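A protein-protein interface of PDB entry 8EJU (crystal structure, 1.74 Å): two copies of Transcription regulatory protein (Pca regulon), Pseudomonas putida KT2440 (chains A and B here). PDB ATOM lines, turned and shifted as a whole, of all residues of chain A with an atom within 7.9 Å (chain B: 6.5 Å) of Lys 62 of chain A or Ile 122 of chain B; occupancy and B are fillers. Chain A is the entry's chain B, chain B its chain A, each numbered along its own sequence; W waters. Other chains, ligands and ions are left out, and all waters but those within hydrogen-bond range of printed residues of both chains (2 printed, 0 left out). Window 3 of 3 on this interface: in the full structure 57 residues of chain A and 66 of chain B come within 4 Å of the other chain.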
ATOM      1  N   PHE A  58      18.114 -16.376  16.922  1.00  0.00           N
ATOM      2  CA  PHE A  58      18.201 -17.459  15.955  1.00  0.00           C
ATOM      3  C   PHE A  58      17.164 -18.533  16.173  1.00  0.00           C
ATOM      4  O   PHE A  58      17.075 -19.421  15.309  1.00  0.00           O
ATOM      5  CB  PHE A  58      19.593 -18.116  15.993  1.00  0.00           C
ATOM      6  CG  PHE A  58      20.637 -17.244  15.359  1.00  0.00           C
ATOM      7  CD1 PHE A  58      21.222 -16.242  16.092  1.00  0.00           C
ATOM      8  CD2 PHE A  58      20.991 -17.406  14.028  1.00  0.00           C
ATOM      9  CE1 PHE A  58      22.163 -15.359  15.471  1.00  0.00           C
ATOM     10  CE2 PHE A  58      21.940 -16.554  13.413  1.00  0.00           C
ATOM     11  CZ  PHE A  58      22.506 -15.553  14.131  1.00  0.00           C
ATOM     12  N   GLN A  59      16.429 -18.506  17.287  1.00  0.00           N
ATOM     13  CA  GLN A  59      15.463 -19.588  17.554  1.00  0.00           C
ATOM     14  C   GLN A  59      14.588 -19.844  16.334  1.00  0.00           C
ATOM     15  O   GLN A  59      13.922 -18.939  15.834  1.00  0.00           O
ATOM     16  CB  GLN A  59      14.541 -19.248  18.726  1.00  0.00           C
ATOM     17  CG  GLN A  59      15.247 -19.131  20.016  1.00  0.00           C
ATOM     18  CD  GLN A  59      15.631 -20.466  20.644  1.00  0.00           C
ATOM     19  OE1 GLN A  59      15.448 -21.549  20.068  1.00  0.00           O
ATOM     20  NE2 GLN A  59      16.154 -20.387  21.860  1.00  0.00           N
ATOM     21  N   GLU A  60      14.565 -21.105  15.885  1.00  0.00           N
ATOM     22  CA  GLU A  60      13.644 -21.546  14.835  1.00  0.00           C
ATOM     23  C   GLU A  60      13.845 -20.745  13.551  1.00  0.00           C
ATOM     24  O   GLU A  60      12.874 -20.428  12.863  1.00  0.00           O
ATOM     25  CB  GLU A  60      12.178 -21.442  15.269  1.00  0.00           C
ATOM     26  CG  GLU A  60      11.824 -22.169  16.573  1.00  0.00           C
ATOM     27  CD  GLU A  60      12.065 -23.654  16.475  1.00  0.00           C
ATOM     28  OE1 GLU A  60      12.117 -24.163  15.331  1.00  0.00           O
ATOM     29  OE2 GLU A  60      12.210 -24.310  17.530  1.00  0.00           O
ATOM     30  N   ARG A  61      15.092 -20.384  13.238  1.00  0.00           N
ATOM     31  CA  ARG A  61      15.422 -19.708  11.977  1.00  0.00           C
ATOM     32  C   ARG A  61      16.428 -20.604  11.248  1.00  0.00           C
ATOM     33  O   ARG A  61      17.622 -20.584  11.559  1.00  0.00           O
ATOM     34  CB  ARG A  61      16.056 -18.345  12.227  1.00  0.00           C
ATOM     35  CG  ARG A  61      15.170 -17.377  12.979  1.00  0.00           C
ATOM     36  CD  ARG A  61      14.036 -16.936  12.085  1.00  0.00           C
ATOM     37  NE  ARG A  61      13.186 -15.929  12.707  1.00  0.00           N
ATOM     38  CZ  ARG A  61      12.118 -16.183  13.454  1.00  0.00           C
ATOM     39  NH1 ARG A  61      11.746 -17.429  13.733  1.00  0.00           N
ATOM     40  NH2 ARG A  61      11.410 -15.159  13.937  1.00  0.00           N
ATOM     41  N   LYS A  62      15.995 -21.321  10.235  1.00  0.00           N
ATOM     42  CA  LYS A  62      16.903 -22.287   9.604  1.00  0.00           C
ATOM     43  C   LYS A  62      17.806 -21.652   8.548  1.00  0.00           C
ATOM     44  O   LYS A  62      18.769 -22.283   8.081  1.00  0.00           O
ATOM     45  CB  LYS A  62      16.075 -23.389   8.934  1.00  0.00           C
ATOM     46  CG  LYS A  62      15.346 -24.376   9.854  1.00  0.00           C
ATOM     47  CD  LYS A  62      14.692 -25.471   8.953  1.00  0.00           C
ATOM     48  CE  LYS A  62      13.364 -26.008   9.495  1.00  0.00           C
ATOM     49  NZ  LYS A  62      13.431 -26.267  10.960  1.00  0.00           N
ATOM     50  N   ARG A  63      17.481 -20.443   8.118  1.00  0.00           N
ATOM     51  CA  ARG A  63      18.285 -19.675   7.179  1.00  0.00           C
ATOM     52  C   ARG A  63      19.119 -18.637   7.930  1.00  0.00           C
ATOM     53  O   ARG A  63      18.693 -18.081   8.951  1.00  0.00           O
ATOM     54  CB  ARG A  63      17.404 -19.033   6.090  1.00  0.00           C
ATOM     55  CG  ARG A  63      16.282 -18.115   6.598  1.00  0.00           C
ATOM     56  CD  ARG A  63      15.372 -18.874   7.621  1.00  0.00           C
ATOM     57  NE  ARG A  63      14.130 -18.224   8.014  1.00  0.00           N
ATOM     58  CZ  ARG A  63      13.180 -18.815   8.726  1.00  0.00           C
ATOM     59  NH1 ARG A  63      13.323 -20.057   9.177  1.00  0.00           N
ATOM     60  NH2 ARG A  63      12.060 -18.148   8.992  1.00  0.00           N
ATOM     61  N   HIS A  64      20.328 -18.398   7.446  1.00  0.00           N
ATOM     62  CA  HIS A  64      21.188 -17.440   8.133  1.00  0.00           C
ATOM     63  C   HIS A  64      20.515 -16.076   8.197  1.00  0.00           C
ATOM     64  O   HIS A  64      19.754 -15.691   7.298  1.00  0.00           O
ATOM     65  CB  HIS A  64      22.521 -17.318   7.406  1.00  0.00           C
ATOM     66  CG  HIS A  64      23.161 -18.634   7.082  1.00  0.00           C
ATOM     67  ND1 HIS A  64      22.827 -19.808   7.732  1.00  0.00           N
ATOM     68  CD2 HIS A  64      24.091 -18.969   6.152  1.00  0.00           C
ATOM     69  CE1 HIS A  64      23.546 -20.801   7.233  1.00  0.00           C
ATOM     70  NE2 HIS A  64      24.319 -20.319   6.273  1.00  0.00           N
ATOM     71  N   LEU A  65      20.854 -15.318   9.218  1.00  0.00           N
ATOM     72  CA  LEU A  65      20.127 -14.095   9.501  1.00  0.00           C
ATOM     73  C   LEU A  65      20.984 -12.874   9.166  1.00  0.00           C
ATOM     74  O   LEU A  65      22.235 -12.915   9.221  1.00  0.00           O
ATOM     75  CB  LEU A  65      19.752 -13.970  10.982  1.00  0.00           C
ATOM     76  CG  LEU A  65      18.801 -15.042  11.560  1.00  0.00           C
ATOM     77  CD1 LEU A  65      18.611 -14.822  13.054  1.00  0.00           C
ATOM     78  CD2 LEU A  65      17.505 -14.955  10.761  1.00  0.00           C
ATOM     79  N   SER A 102      25.357 -16.946  11.277  1.00  0.00           N
ATOM     80  CA  SER A 102      24.842 -18.189  11.837  1.00  0.00           C
ATOM     81  C   SER A 102      25.503 -18.424  13.188  1.00  0.00           C
ATOM     82  O   SER A 102      26.533 -17.824  13.509  1.00  0.00           O
ATOM     83  CB  SER A 102      25.110 -19.395  10.905  1.00  0.00           C
ATOM     84  OG  SER A 102      24.410 -19.262   9.670  1.00  0.00           O
ATOM     85  N   SER A 163       6.537 -34.944  13.981  1.00  0.00           N
ATOM     86  CA  SER A 163       7.713 -35.637  13.437  1.00  0.00           C
ATOM     87  C   SER A 163       9.042 -34.935  13.767  1.00  0.00           C
ATOM     88  O   SER A 163      10.042 -35.129  13.074  1.00  0.00           O
ATOM     89  CB  SER A 163       7.570 -35.863  11.919  1.00  0.00           C
ATOM     90  OG  SER A 163       7.958 -34.728  11.160  1.00  0.00           O
ATOM     91  N   VAL A 164       9.100 -34.146  14.837  1.00  0.00           N
ATOM     92  CA  VAL A 164      10.338 -33.515  15.286  1.00  0.00           C
ATOM     93  C   VAL A 164      10.578 -33.919  16.737  1.00  0.00           C
ATOM     94  O   VAL A 164       9.681 -33.784  17.580  1.00  0.00           O
ATOM     95  CB  VAL A 164      10.279 -31.983  15.124  1.00  0.00           C
ATOM     96  CG1 VAL A 164      11.574 -31.325  15.603  1.00  0.00           C
ATOM     97  CG2 VAL A 164      10.021 -31.630  13.654  1.00  0.00           C
ATOM     98  N   ASP A 165      11.776 -34.443  17.022  1.00  0.00           N
ATOM     99  CA  ASP A 165      12.077 -34.916  18.373  1.00  0.00           C
ATOM    100  C   ASP A 165      11.990 -33.743  19.345  1.00  0.00           C
ATOM    101  O   ASP A 165      12.461 -32.641  19.048  1.00  0.00           O
ATOM    102  CB  ASP A 165      13.481 -35.557  18.453  1.00  0.00           C
ATOM    103  CG  ASP A 165      13.592 -36.883  17.704  1.00  0.00           C
ATOM    104  OD1 ASP A 165      12.705 -37.175  16.879  1.00  0.00           O
ATOM    105  OD2 ASP A 165      14.606 -37.617  17.898  1.00  0.00           O
ATOM    106  N   TYR B 114      20.855 -22.684  18.611  1.00  0.00           N
ATOM    107  CA  TYR B 114      21.716 -23.303  17.607  1.00  0.00           C
ATOM    108  C   TYR B 114      21.029 -24.511  17.009  1.00  0.00           C
ATOM    109  O   TYR B 114      20.953 -24.657  15.785  1.00  0.00           O
ATOM    110  CB  TYR B 114      23.065 -23.703  18.249  1.00  0.00           C
ATOM    111  CG  TYR B 114      23.851 -24.620  17.332  1.00  0.00           C
ATOM    112  CD1 TYR B 114      24.604 -24.109  16.232  1.00  0.00           C
ATOM    113  CD2 TYR B 114      23.737 -26.004  17.437  1.00  0.00           C
ATOM    114  CE1 TYR B 114      25.248 -24.958  15.355  1.00  0.00           C
ATOM    115  CE2 TYR B 114      24.401 -26.847  16.576  1.00  0.00           C
ATOM    116  CZ  TYR B 114      25.146 -26.331  15.530  1.00  0.00           C
ATOM    117  OH  TYR B 114      25.778 -27.178  14.681  1.00  0.00           O
ATOM    118  N   LEU B 115      20.461 -25.370  17.853  1.00  0.00           N
ATOM    119  CA  LEU B 115      19.923 -26.607  17.293  1.00  0.00           C
ATOM    120  C   LEU B 115      18.795 -26.320  16.326  1.00  0.00           C
ATOM    121  O   LEU B 115      18.667 -26.989  15.303  1.00  0.00           O
ATOM    122  CB  LEU B 115      19.430 -27.551  18.409  1.00  0.00           C
ATOM    123  CG  LEU B 115      20.568 -28.102  19.282  1.00  0.00           C
ATOM    124  CD1 LEU B 115      19.975 -28.773  20.519  1.00  0.00           C
ATOM    125  CD2 LEU B 115      21.555 -29.042  18.505  1.00  0.00           C
ATOM    126  N   SER B 116      17.948 -25.341  16.651  1.00  0.00           N
ATOM    127  CA  SER B 116      16.760 -25.115  15.855  1.00  0.00           C
ATOM    128  C   SER B 116      17.027 -24.229  14.646  1.00  0.00           C
ATOM    129  O   SER B 116      16.102 -23.941  13.884  1.00  0.00           O
ATOM    130  CB  SER B 116      15.665 -24.501  16.716  1.00  0.00           C
ATOM    131  OG  SER B 116      16.007 -23.187  17.206  1.00  0.00           O
ATOM    132  N   SER B 117      18.259 -23.789  14.474  1.00  0.00           N
ATOM    133  CA  SER B 117      18.634 -22.968  13.333  1.00  0.00           C
ATOM    134  C   SER B 117      19.681 -23.650  12.483  1.00  0.00           C
ATOM    135  O   SER B 117      20.172 -23.057  11.511  1.00  0.00           O
ATOM    136  CB  SER B 117      19.122 -21.594  13.822  1.00  0.00           C
ATOM    137  OG  SER B 117      20.347 -21.687  14.574  1.00  0.00           O
ATOM    138  N   THR B 118      19.962 -24.924  12.745  1.00  0.00           N
ATOM    139  CA  THR B 118      20.997 -25.655  12.005  1.00  0.00           C
ATOM    140  C   THR B 118      20.490 -26.892  11.288  1.00  0.00           C
ATOM    141  O   THR B 118      20.310 -27.950  11.923  1.00  0.00           O
ATOM    142  CB  THR B 118      22.069 -26.082  12.993  1.00  0.00           C
ATOM    143  OG1 THR B 118      22.581 -24.911  13.624  1.00  0.00           O
ATOM    144  CG2 THR B 118      23.213 -26.852  12.267  1.00  0.00           C
ATOM    145  N   PRO B 119      20.305 -26.845   9.958  1.00  0.00           N
ATOM    146  CA  PRO B 119      19.728 -28.024   9.280  1.00  0.00           C
ATOM    147  C   PRO B 119      20.531 -29.293   9.442  1.00  0.00           C
ATOM    148  O   PRO B 119      19.932 -30.370   9.514  1.00  0.00           O
ATOM    149  CB  PRO B 119      19.625 -27.572   7.812  1.00  0.00           C
ATOM    150  CG  PRO B 119      19.437 -26.083   7.895  1.00  0.00           C
ATOM    151  CD  PRO B 119      20.337 -25.662   9.073  1.00  0.00           C
ATOM    152  N   LEU B 120      21.854 -29.215   9.602  1.00  0.00           N
ATOM    153  CA  LEU B 120      22.631 -30.431   9.778  1.00  0.00           C
ATOM    154  C   LEU B 120      22.192 -31.194  11.022  1.00  0.00           C
ATOM    155  O   LEU B 120      21.958 -32.395  10.965  1.00  0.00           O
ATOM    156  CB  LEU B 120      24.115 -30.071   9.846  1.00  0.00           C
ATOM    157  CG  LEU B 120      25.015 -31.226  10.229  1.00  0.00           C
ATOM    158  CD1 LEU B 120      24.838 -32.366   9.257  1.00  0.00           C
ATOM    159  CD2 LEU B 120      26.451 -30.664  10.311  1.00  0.00           C
ATOM    160  N   ALA B 121      22.019 -30.490  12.145  1.00  0.00           N
ATOM    161  CA  ALA B 121      21.615 -31.122  13.399  1.00  0.00           C
ATOM    162  C   ALA B 121      20.182 -31.617  13.308  1.00  0.00           C
ATOM    163  O   ALA B 121      19.869 -32.712  13.782  1.00  0.00           O
ATOM    164  CB  ALA B 121      21.741 -30.080  14.538  1.00  0.00           C
ATOM    165  N   ILE B 122      19.314 -30.813  12.690  1.00  0.00           N
ATOM    166  CA  ILE B 122      17.897 -31.165  12.574  1.00  0.00           C
ATOM    167  C   ILE B 122      17.738 -32.404  11.703  1.00  0.00           C
ATOM    168  O   ILE B 122      17.073 -33.376  12.078  1.00  0.00           O
ATOM    169  CB  ILE B 122      17.085 -29.984  12.018  1.00  0.00           C
ATOM    170  CG1 ILE B 122      17.152 -28.749  12.953  1.00  0.00           C
ATOM    171  CG2 ILE B 122      15.588 -30.364  11.781  1.00  0.00           C
ATOM    172  CD1 ILE B 122      16.707 -27.419  12.260  1.00  0.00           C
ATOM    173  N   SER B 123      18.372 -32.397  10.534  1.00  0.00           N
ATOM    174  CA  SER B 123      18.191 -33.505   9.591  1.00  0.00           C
ATOM    175  C   SER B 123      18.929 -34.752  10.014  1.00  0.00           C
ATOM    176  O   SER B 123      18.607 -35.853   9.525  1.00  0.00           O
ATOM    177  CB  SER B 123      18.672 -33.073   8.227  1.00  0.00           C
ATOM    178  OG  SER B 123      17.833 -32.019   7.807  1.00  0.00           O
ATOM    179  N   ALA B 124      19.937 -34.614  10.877  1.00  0.00           N
ATOM    180  CA  ALA B 124      20.676 -35.795  11.309  1.00  0.00           C
ATOM    181  C   ALA B 124      19.849 -36.674  12.239  1.00  0.00           C
ATOM    182  O   ALA B 124      20.030 -37.900  12.233  1.00  0.00           O
ATOM    183  CB  ALA B 124      21.987 -35.413  11.998  1.00  0.00           C
ATOM    184  N   GLN B 125      18.884 -36.093  12.952  1.00  0.00           N
ATOM    185  CA  GLN B 125      18.226 -36.800  14.057  1.00  0.00           C
ATOM    186  C   GLN B 125      17.459 -38.045  13.618  1.00  0.00           C
ATOM    187  O   GLN B 125      17.603 -39.090  14.276  1.00  0.00           O
ATOM    188  CB  GLN B 125      17.318 -35.850  14.846  1.00  0.00           C
ATOM    189  CG  GLN B 125      16.878 -36.475  16.161  1.00  0.00           C
ATOM    190  CD  GLN B 125      18.027 -36.631  17.168  1.00  0.00           C
ATOM    191  OE1 GLN B 125      18.831 -35.709  17.389  1.00  0.00           O
ATOM    192  NE2 GLN B 125      18.100 -37.798  17.795  1.00  0.00           N
ATOM    193  N   PRO B 126      16.614 -38.018  12.575  1.00  0.00           N
ATOM    194  CA  PRO B 126      15.960 -39.271  12.152  1.00  0.00           C
ATOM    195  C   PRO B 126      16.917 -40.385  11.768  1.00  0.00           C
ATOM    196  O   PRO B 126      16.601 -41.565  11.965  1.00  0.00           O
ATOM    197  CB  PRO B 126      15.123 -38.844  10.929  1.00  0.00           C
ATOM    198  CG  PRO B 126      14.960 -37.384  11.055  1.00  0.00           C
ATOM    199  CD  PRO B 126      16.187 -36.868  11.745  1.00  0.00           C
ATOM    200  N   MET B 141      26.564 -37.684  16.504  1.00  0.00           N
ATOM    201  CA  MET B 141      27.213 -36.832  15.528  1.00  0.00           C
ATOM    202  C   MET B 141      27.906 -35.674  16.213  1.00  0.00           C
ATOM    203  O   MET B 141      27.390 -35.101  17.177  1.00  0.00           O
ATOM    204  CB  MET B 141      26.278 -36.408  14.386  1.00  0.00           C
ATOM    205  CG  MET B 141      26.828 -35.340  13.496  1.00  0.00           C
ATOM    206  SD  MET B 141      25.591 -34.780  12.292  1.00  0.00           S
ATOM    207  CE  MET B 141      24.695 -33.484  13.093  1.00  0.00           C
ATOM    208  N   ALA B 153      24.432 -33.977  18.105  1.00  0.00           N
ATOM    209  CA  ALA B 153      23.165 -34.729  18.129  1.00  0.00           C
ATOM    210  C   ALA B 153      23.440 -36.169  18.591  1.00  0.00           C
ATOM    211  O   ALA B 153      24.509 -36.725  18.385  1.00  0.00           O
ATOM    212  CB  ALA B 153      22.490 -34.737  16.747  1.00  0.00           C
HETATM  213  O   HOH W   1      21.569 -22.030   9.100  1.00  0.00           O
HETATM  214  O   HOH W   2      13.948 -25.043  13.267  1.00  0.00           O
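The side-chain amide nitrogen (NE2) of Gln 125 of chain B lies close to the side-chain carboxylate (OD2) of Asp 165 of chain A (3.5 Å). The backbone NH (N) of Glu 60 of chain A lies within hydrogen-bond range of the side-chain hydroxyl (OG) of Ser 116 of chain B (2.9 Å). The side-chain hydroxyl (OG) of Ser 116 of chain B is in hydrogen-bond range of the side-chain amide oxygen (OE1) of Gln 59 of chain A (3.3 Å).
Of the printed residues of chain B, Glu 60 of chain A touches Ser 116. Of chain B, only Ser 117, Pro 119 and Ile 122 come within 4 Å of Lys 62 of chain A. Of the printed residues of chain B, Asp 165 of chain A touches Gln 125 (3.1 Å). Of the printed residues of chain A, Ser 117 of chain B touches Phe 58 (3.3 Å), Arg 61 (2.9 Å) and Lys 62 (3.8 Å). Printed residues of chain A within 4 Å of Pro 119 of chain B: Lys 62 (3.9 Å). No residue of chain A comes within 4 Å of Ala 121 of chain B. Of chain A, only Lys 62 comes within 4 Å of Ile 122 of chain B. Pro 126 of chain B touches none of the printed residues of chain A. The nearest residue of chain B that does not touch Lys 62 of chain A is Ser 116 of chain B (4.1 Å). The nearest residue of chain A that does not touch Ile 122 of chain B is Val 164 of chain A (5.6 Å). The nearest printed residue of chain B that does not touch Glu 60 of chain A is Ser 117 of chain B (4.8 Å).
Water W2 lies within hydrogen-bond range of the backbone carbonyl oxygen (O) of Ser 116 of chain B (2.5 Å), the side-chain amino group (NZ) of Lys 62 of chain A (2.7 Å) and the side-chain carboxylate (OE1) of Glu 60 of chain A (2.9 Å). Water W1 lies within hydrogen-bond range of ND1 of His 64 of chain A (2.9 Å), O of Ser 117 of chain B (3.0 Å) and O of Lys 62 of chain A (3.0 Å).
The backbone carbonyl oxygen (O) of Tyr 114 of chain B lies within hydrogen-bond range of the side-chain hydroxyl (OG) of Ser 117 of chain B (3.3 Å). O of Gln 59 of chain A is in hydrogen-bond range of NH1 of Arg 61 of chain A. The backbone carbonyl oxygen of Pro 119 of chain B sits at hydrogen-bond distance from the side-chain hydroxyl of Ser 123 of chain B (3.2 Å).
Of the 12 printed residues of chain A, 6 touch a printed residue of chain B. Hydrophobic or aromatic side chains of chain A that line the printed part of chain B: Phe 58. Among the printed residues, no Asp or Glu carboxylate lies within 4 Å of a Lys or Arg side-chain nitrogen of the other chain.
Among the printed residues, merely in contact across the chains: Arg 61 of chain A with Ser 117 of chain B (2.9 Å), Phe 58 of chain A with Ser 117 of chain B (3.3 Å), Lys 62 of chain A with Ile 122 of chain B (3.7 Å), Arg 61 of chain A with Ser 116 of chain B (3.8 Å), Lys 62 of chain A with Ser 117 of chain B (3.8 Å) and Lys 62 of chain A with Pro 119 of chain B (3.9 Å).
No position is printed for both chains. Of the 9 pairs that touch across the chains among the printed residues, none has its exchanged pair printed and touching as well.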
